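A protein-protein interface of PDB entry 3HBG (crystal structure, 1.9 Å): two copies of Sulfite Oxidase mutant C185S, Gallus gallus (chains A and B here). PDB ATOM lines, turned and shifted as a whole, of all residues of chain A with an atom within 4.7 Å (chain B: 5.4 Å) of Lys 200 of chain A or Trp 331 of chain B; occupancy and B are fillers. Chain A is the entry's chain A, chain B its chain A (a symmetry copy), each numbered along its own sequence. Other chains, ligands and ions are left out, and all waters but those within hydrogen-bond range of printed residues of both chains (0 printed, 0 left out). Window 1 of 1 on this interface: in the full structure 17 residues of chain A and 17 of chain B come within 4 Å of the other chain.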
ATOM      1  N   ARG A 190      33.067 -20.155 -21.444  1.00  0.00           N
ATOM      2  CA  ARG A 190      31.779 -20.575 -22.020  1.00  0.00           C
ATOM      3  C   ARG A 190      31.467 -19.859 -23.344  1.00  0.00           C
ATOM      4  O   ARG A 190      30.911 -20.477 -24.261  1.00  0.00           O
ATOM      5  CB  ARG A 190      30.625 -20.371 -21.024  1.00  0.00           C
ATOM      6  CG  ARG A 190      29.251 -20.734 -21.597  1.00  0.00           C
ATOM      7  CD  ARG A 190      28.146 -20.651 -20.551  1.00  0.00           C
ATOM      8  NE  ARG A 190      28.189 -21.766 -19.603  1.00  0.00           N
ATOM      9  CZ  ARG A 190      28.267 -21.650 -18.282  1.00  0.00           C
ATOM     10  NH1 ARG A 190      28.310 -20.453 -17.696  1.00  0.00           N
ATOM     11  NH2 ARG A 190      28.285 -22.750 -17.533  1.00  0.00           N
ATOM     12  N   PRO A 198      24.553 -22.232 -29.508  1.00  0.00           N
ATOM     13  CA  PRO A 198      24.025 -21.574 -28.309  1.00  0.00           C
ATOM     14  C   PRO A 198      23.953 -22.509 -27.101  1.00  0.00           C
ATOM     15  O   PRO A 198      23.574 -23.672 -27.245  1.00  0.00           O
ATOM     16  CB  PRO A 198      22.618 -21.150 -28.734  1.00  0.00           C
ATOM     17  CG  PRO A 198      22.715 -20.965 -30.208  1.00  0.00           C
ATOM     18  CD  PRO A 198      23.692 -21.996 -30.689  1.00  0.00           C
ATOM     19  N   VAL A 199      24.336 -21.995 -25.933  1.00  0.00           N
ATOM     20  CA  VAL A 199      24.308 -22.757 -24.681  1.00  0.00           C
ATOM     21  C   VAL A 199      23.487 -22.055 -23.607  1.00  0.00           C
ATOM     22  O   VAL A 199      23.093 -20.904 -23.771  1.00  0.00           O
ATOM     23  CB  VAL A 199      25.733 -23.005 -24.104  1.00  0.00           C
ATOM     24  CG1 VAL A 199      26.614 -23.751 -25.092  1.00  0.00           C
ATOM     25  CG2 VAL A 199      26.387 -21.691 -23.662  1.00  0.00           C
ATOM     26  N   LYS A 200      23.251 -22.757 -22.499  1.00  0.00           N
ATOM     27  CA  LYS A 200      22.631 -22.176 -21.318  1.00  0.00           C
ATOM     28  C   LYS A 200      23.691 -21.818 -20.295  1.00  0.00           C
ATOM     29  O   LYS A 200      24.570 -22.637 -19.981  1.00  0.00           O
ATOM     30  CB  LYS A 200      21.652 -23.159 -20.681  1.00  0.00           C
ATOM     31  CG  LYS A 200      20.343 -23.343 -21.423  1.00  0.00           C
ATOM     32  CD  LYS A 200      19.547 -24.513 -20.832  1.00  0.00           C
ATOM     33  CE  LYS A 200      19.316 -24.347 -19.326  1.00  0.00           C
ATOM     34  NZ  LYS A 200      18.212 -23.393 -19.025  1.00  0.00           N
ATOM     35  N   GLY A 201      23.598 -20.604 -19.761  1.00  0.00           N
ATOM     36  CA  GLY A 201      24.520 -20.142 -18.725  1.00  0.00           C
ATOM     37  C   GLY A 201      25.160 -18.804 -19.064  1.00  0.00           C
ATOM     38  O   GLY A 201      25.150 -18.371 -20.220  1.00  0.00           O
ATOM     39  N   LEU A 449      25.576 -28.607 -23.835  1.00  0.00           N
ATOM     40  CA  LEU A 449      24.515 -27.604 -23.655  1.00  0.00           C
ATOM     41  C   LEU A 449      24.749 -26.647 -22.478  1.00  0.00           C
ATOM     42  O   LEU A 449      24.373 -25.474 -22.541  1.00  0.00           O
ATOM     43  CB  LEU A 449      23.138 -28.269 -23.521  1.00  0.00           C
ATOM     44  CG  LEU A 449      21.920 -27.328 -23.447  1.00  0.00           C
ATOM     45  CD1 LEU A 449      21.814 -26.422 -24.691  1.00  0.00           C
ATOM     46  CD2 LEU A 449      20.620 -28.102 -23.229  1.00  0.00           C
ATOM     47  N   ARG A 450      25.356 -27.153 -21.410  1.00  0.00           N
ATOM     48  CA  ARG A 450      25.652 -26.328 -20.232  1.00  0.00           C
ATOM     49  C   ARG A 450      26.861 -25.409 -20.431  1.00  0.00           C
ATOM     50  O   ARG A 450      27.111 -24.521 -19.609  1.00  0.00           O
ATOM     51  CB  ARG A 450      25.869 -27.209 -19.000  1.00  0.00           C
ATOM     52  CG  ARG A 450      24.609 -27.905 -18.489  1.00  0.00           C
ATOM     53  CD  ARG A 450      24.927 -28.739 -17.243  1.00  0.00           C
ATOM     54  NE  ARG A 450      25.574 -27.934 -16.200  1.00  0.00           N
ATOM     55  CZ  ARG A 450      26.490 -28.387 -15.344  1.00  0.00           C
ATOM     56  NH1 ARG A 450      26.893 -29.652 -15.391  1.00  0.00           N
ATOM     57  NH2 ARG A 450      27.013 -27.568 -14.440  1.00  0.00           N
ATOM     58  N   GLY A 451      27.604 -25.634 -21.515  1.00  0.00           N
ATOM     59  CA  GLY A 451      28.781 -24.831 -21.848  1.00  0.00           C
ATOM     60  C   GLY A 451      29.875 -24.876 -20.795  1.00  0.00           C
ATOM     61  O   GLY A 451      30.577 -23.882 -20.584  1.00  0.00           O
ATOM     62  N   HIS B 140      10.815 -16.834 -17.286  1.00  0.00           N
ATOM     63  CA  HIS B 140      12.202 -17.208 -16.981  1.00  0.00           C
ATOM     64  C   HIS B 140      13.149 -16.029 -17.205  1.00  0.00           C
ATOM     65  O   HIS B 140      14.217 -15.942 -16.580  1.00  0.00           O
ATOM     66  CB  HIS B 140      12.654 -18.382 -17.861  1.00  0.00           C
ATOM     67  CG  HIS B 140      12.109 -19.712 -17.437  1.00  0.00           C
ATOM     68  ND1 HIS B 140      10.829 -20.124 -17.738  1.00  0.00           N
ATOM     69  CD2 HIS B 140      12.681 -20.734 -16.753  1.00  0.00           C
ATOM     70  CE1 HIS B 140      10.626 -21.333 -17.242  1.00  0.00           C
ATOM     71  NE2 HIS B 140      11.737 -21.728 -16.642  1.00  0.00           N
ATOM     72  N   LEU B 141      12.738 -15.124 -18.089  1.00  0.00           N
ATOM     73  CA  LEU B 141      13.624 -14.113 -18.664  1.00  0.00           C
ATOM     74  C   LEU B 141      12.897 -12.769 -18.833  1.00  0.00           C
ATOM     75  O   LEU B 141      11.692 -12.682 -18.552  1.00  0.00           O
ATOM     76  CB  LEU B 141      14.136 -14.629 -20.019  1.00  0.00           C
ATOM     77  CG  LEU B 141      15.040 -15.874 -19.953  1.00  0.00           C
ATOM     78  CD1 LEU B 141      15.039 -16.641 -21.276  1.00  0.00           C
ATOM     79  CD2 LEU B 141      16.463 -15.512 -19.531  1.00  0.00           C
ATOM     80  N   ALA B 245      15.828 -15.366 -24.775  1.00  0.00           N
ATOM     81  CA  ALA B 245      17.010 -16.221 -24.766  1.00  0.00           C
ATOM     82  C   ALA B 245      17.861 -16.068 -23.506  1.00  0.00           C
ATOM     83  O   ALA B 245      18.003 -14.969 -22.970  1.00  0.00           O
ATOM     84  CB  ALA B 245      17.855 -15.971 -26.021  1.00  0.00           C
ATOM     85  N   ASP B 246      18.408 -17.193 -23.050  1.00  0.00           N
ATOM     86  CA  ASP B 246      19.434 -17.237 -21.992  1.00  0.00           C
ATOM     87  C   ASP B 246      20.625 -16.370 -22.406  1.00  0.00           C
ATOM     88  O   ASP B 246      20.893 -16.229 -23.601  1.00  0.00           O
ATOM     89  CB  ASP B 246      19.874 -18.697 -21.777  1.00  0.00           C
ATOM     90  CG  ASP B 246      20.738 -18.888 -20.543  1.00  0.00           C
ATOM     91  OD1 ASP B 246      21.961 -18.656 -20.628  1.00  0.00           O
ATOM     92  OD2 ASP B 246      20.195 -19.304 -19.494  1.00  0.00           O
ATOM     93  N   GLY B 248      23.568 -17.162 -22.395  1.00  0.00           N
ATOM     94  CA  GLY B 248      24.468 -18.041 -23.158  1.00  0.00           C
ATOM     95  C   GLY B 248      24.046 -18.238 -24.610  1.00  0.00           C
ATOM     96  O   GLY B 248      24.814 -18.769 -25.421  1.00  0.00           O
ATOM     97  N   ALA B 250      20.936 -19.774 -25.726  1.00  0.00           N
ATOM     98  CA  ALA B 250      19.839 -20.720 -25.895  1.00  0.00           C
ATOM     99  C   ALA B 250      18.477 -20.064 -25.623  1.00  0.00           C
ATOM    100  O   ALA B 250      18.264 -19.504 -24.548  1.00  0.00           O
ATOM    101  CB  ALA B 250      20.041 -21.941 -24.996  1.00  0.00           C
ATOM    102  N   PRO B 251      17.556 -20.121 -26.605  1.00  0.00           N
ATOM    103  CA  PRO B 251      16.185 -19.630 -26.372  1.00  0.00           C
ATOM    104  C   PRO B 251      15.450 -20.531 -25.392  1.00  0.00           C
ATOM    105  O   PRO B 251      15.784 -21.718 -25.289  1.00  0.00           O
ATOM    106  CB  PRO B 251      15.510 -19.755 -27.752  1.00  0.00           C
ATOM    107  CG  PRO B 251      16.588 -20.151 -28.717  1.00  0.00           C
ATOM    108  CD  PRO B 251      17.719 -20.736 -27.935  1.00  0.00           C
ATOM    109  N   TYR B 252      14.458 -19.994 -24.677  1.00  0.00           N
ATOM    110  CA  TYR B 252      13.550 -20.878 -23.947  1.00  0.00           C
ATOM    111  C   TYR B 252      12.900 -21.801 -24.968  1.00  0.00           C
ATOM    112  O   TYR B 252      12.482 -21.365 -26.049  1.00  0.00           O
ATOM    113  CB  TYR B 252      12.465 -20.139 -23.152  1.00  0.00           C
ATOM    114  CG  TYR B 252      11.595 -21.117 -22.374  1.00  0.00           C
ATOM    115  CD1 TYR B 252      12.003 -21.594 -21.128  1.00  0.00           C
ATOM    116  CD2 TYR B 252      10.400 -21.611 -22.915  1.00  0.00           C
ATOM    117  CE1 TYR B 252      11.235 -22.523 -20.422  1.00  0.00           C
ATOM    118  CE2 TYR B 252       9.613 -22.535 -22.207  1.00  0.00           C
ATOM    119  CZ  TYR B 252      10.039 -22.981 -20.965  1.00  0.00           C
ATOM    120  OH  TYR B 252       9.292 -23.896 -20.254  1.00  0.00           O
ATOM    121  N   GLY B 253      12.835 -23.079 -24.630  1.00  0.00           N
ATOM    122  CA  GLY B 253      12.266 -24.066 -25.530  1.00  0.00           C
ATOM    123  C   GLY B 253      11.598 -25.189 -24.769  1.00  0.00           C
ATOM    124  O   GLY B 253      11.902 -25.415 -23.588  1.00  0.00           O
ATOM    125  N   ALA B 254      10.683 -25.875 -25.453  1.00  0.00           N
ATOM    126  CA  ALA B 254      10.038 -27.082 -24.938  1.00  0.00           C
ATOM    127  C   ALA B 254       9.532 -27.901 -26.123  1.00  0.00           C
ATOM    128  O   ALA B 254       9.398 -27.378 -27.232  1.00  0.00           O
ATOM    129  CB  ALA B 254       8.897 -26.720 -23.994  1.00  0.00           C
ATOM    130  N   VAL B 329      16.244 -27.162 -28.485  1.00  0.00           N
ATOM    131  CA  VAL B 329      16.422 -27.808 -27.179  1.00  0.00           C
ATOM    132  C   VAL B 329      15.325 -27.497 -26.156  1.00  0.00           C
ATOM    133  O   VAL B 329      15.013 -26.334 -25.884  1.00  0.00           O
ATOM    134  CB  VAL B 329      17.830 -27.535 -26.564  1.00  0.00           C
ATOM    135  CG1 VAL B 329      18.899 -28.311 -27.319  1.00  0.00           C
ATOM    136  CG2 VAL B 329      18.152 -26.038 -26.539  1.00  0.00           C
ATOM    137  N   ASP B 330      14.741 -28.563 -25.608  1.00  0.00           N
ATOM    138  CA  ASP B 330      13.808 -28.480 -24.488  1.00  0.00           C
ATOM    139  C   ASP B 330      14.622 -28.179 -23.221  1.00  0.00           C
ATOM    140  O   ASP B 330      15.565 -28.905 -22.896  1.00  0.00           O
ATOM    141  CB  ASP B 330      13.015 -29.797 -24.369  1.00  0.00           C
ATOM    142  CG  ASP B 330      12.035 -29.809 -23.196  1.00  0.00           C
ATOM    143  OD1 ASP B 330      12.489 -29.933 -22.039  1.00  0.00           O
ATOM    144  OD2 ASP B 330      10.806 -29.736 -23.428  1.00  0.00           O
ATOM    145  N   TRP B 331      14.250 -27.103 -22.527  1.00  0.00           N
ATOM    146  CA  TRP B 331      15.009 -26.570 -21.380  1.00  0.00           C
ATOM    147  C   TRP B 331      15.235 -27.518 -20.194  1.00  0.00           C
ATOM    148  O   TRP B 331      16.072 -27.238 -19.328  1.00  0.00           O
ATOM    149  CB  TRP B 331      14.380 -25.253 -20.898  1.00  0.00           C
ATOM    150  CG  TRP B 331      15.094 -24.008 -21.382  1.00  0.00           C
ATOM    151  CD1 TRP B 331      15.632 -23.785 -22.627  1.00  0.00           C
ATOM    152  CD2 TRP B 331      15.334 -22.811 -20.629  1.00  0.00           C
ATOM    153  NE1 TRP B 331      16.197 -22.529 -22.691  1.00  0.00           N
ATOM    154  CE2 TRP B 331      16.023 -21.907 -21.481  1.00  0.00           C
ATOM    155  CE3 TRP B 331      15.027 -22.412 -19.317  1.00  0.00           C
ATOM    156  CZ2 TRP B 331      16.420 -20.631 -21.062  1.00  0.00           C
ATOM    157  CZ3 TRP B 331      15.419 -21.143 -18.902  1.00  0.00           C
ATOM    158  CH2 TRP B 331      16.109 -20.268 -19.774  1.00  0.00           C
ATOM    159  N   ASP B 332      14.512 -28.637 -20.161  1.00  0.00           N
ATOM    160  CA  ASP B 332      14.683 -29.638 -19.098  1.00  0.00           C
ATOM    161  C   ASP B 332      16.027 -30.374 -19.151  1.00  0.00           C
ATOM    162  O   ASP B 332      16.424 -31.012 -18.171  1.00  0.00           O
ATOM    163  CB  ASP B 332      13.532 -30.648 -19.110  1.00  0.00           C
ATOM    164  CG  ASP B 332      12.211 -30.036 -18.680  1.00  0.00           C
ATOM    165  OD1 ASP B 332      12.014 -28.816 -18.867  1.00  0.00           O
ATOM    166  OD2 ASP B 332      11.361 -30.782 -18.154  1.00  0.00           O
ATOM    167  N   THR B 333      16.719 -30.280 -20.287  1.00  0.00           N
ATOM    168  CA  THR B 333      18.025 -30.920 -20.456  1.00  0.00           C
ATOM    169  C   THR B 333      19.108 -30.136 -19.719  1.00  0.00           C
ATOM    170  O   THR B 333      19.977 -30.716 -19.067  1.00  0.00           O
ATOM    171  CB  THR B 333      18.413 -31.044 -21.948  1.00  0.00           C
ATOM    172  OG1 THR B 333      17.241 -31.289 -22.738  1.00  0.00           O
ATOM    173  CG2 THR B 333      19.417 -32.176 -22.155  1.00  0.00           C
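The backbone NH (N) of Val 199 of chain A sits at hydrogen-bond distance from the backbone carbonyl oxygen (O) of Gly 248 of chain B, at 3.3 Å. The backbone NH (N) of Ala 250 of chain B sits at hydrogen-bond distance from the backbone carbonyl oxygen (O) of Val 199 of chain A, 3.1 Å away. The backbone NH of Gly 201 of chain A sits at hydrogen-bond distance from the side-chain carboxylate of Asp 246 of chain B, at 2.7 Å. The backbone NH (N) of Gly 248 of chain B lies within hydrogen-bond range of the backbone carbonyl oxygen (O) of Gly 201 of chain A (2.9 Å).
The backbone carbonyl oxygen of Leu 449 of chain A lies within hydrogen-bond range of the backbone NH of Lys 200 of chain A, 2.9 Å away. The side-chain carboxylate of Asp 246 of chain B sits at hydrogen-bond distance from the backbone NH of Gly 248 of chain B. The backbone carbonyl oxygen (O) of Pro 251 of chain B sits at hydrogen-bond distance from the indole nitrogen (NE1) of Trp 331 of chain B (2.8 Å). The backbone carbonyl oxygen (O) of Gly 253 of chain B is in hydrogen-bond range of the backbone NH (N) of Trp 331 of chain B, at 3.1 Å. The side-chain hydroxyl of Thr 333 of chain B lies within hydrogen-bond range of the backbone carbonyl oxygen of Asp 330 of chain B, at 2.9 Å.
Among the printed residues, pairs that only touch across the chains: Pro 198 of chain A with Ala 250 of chain B (3.7 Å), Lys 200 of chain A with Asp 246 of chain B (3.6 Å), Lys 200 of chain A with Ala 250 of chain B (3.9 Å), Lys 200 of chain A with Trp 331 of chain B (3.3 Å) and Leu 449 of chain A with Thr 333 of chain B (3.9 Å).
Trp 331 of chain B touches just one residue of chain A: Lys 200. Of the printed residues of chain A, Thr 333 of chain B touches Leu 449. Of the printed residues of chain A, Asp 246 of chain B touches Lys 200 and Gly 201. Printed residues of chain B within 4 Å of Gly 201 of chain A: Asp 246 (2.7 Å) and Gly 248 (2.9 Å). Printed residues of chain A within 4 Å of Gly 248 of chain B: Val 199 (3.0 Å) and Gly 201 (2.9 Å). Pro 251 of chain B touches none of the printed residues of chain A.
Among the printed residues, no Asp or Glu carboxylate lies within 4 Å of a Lys or Arg side-chain nitrogen of the other chain.
No position is printed for both chains.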
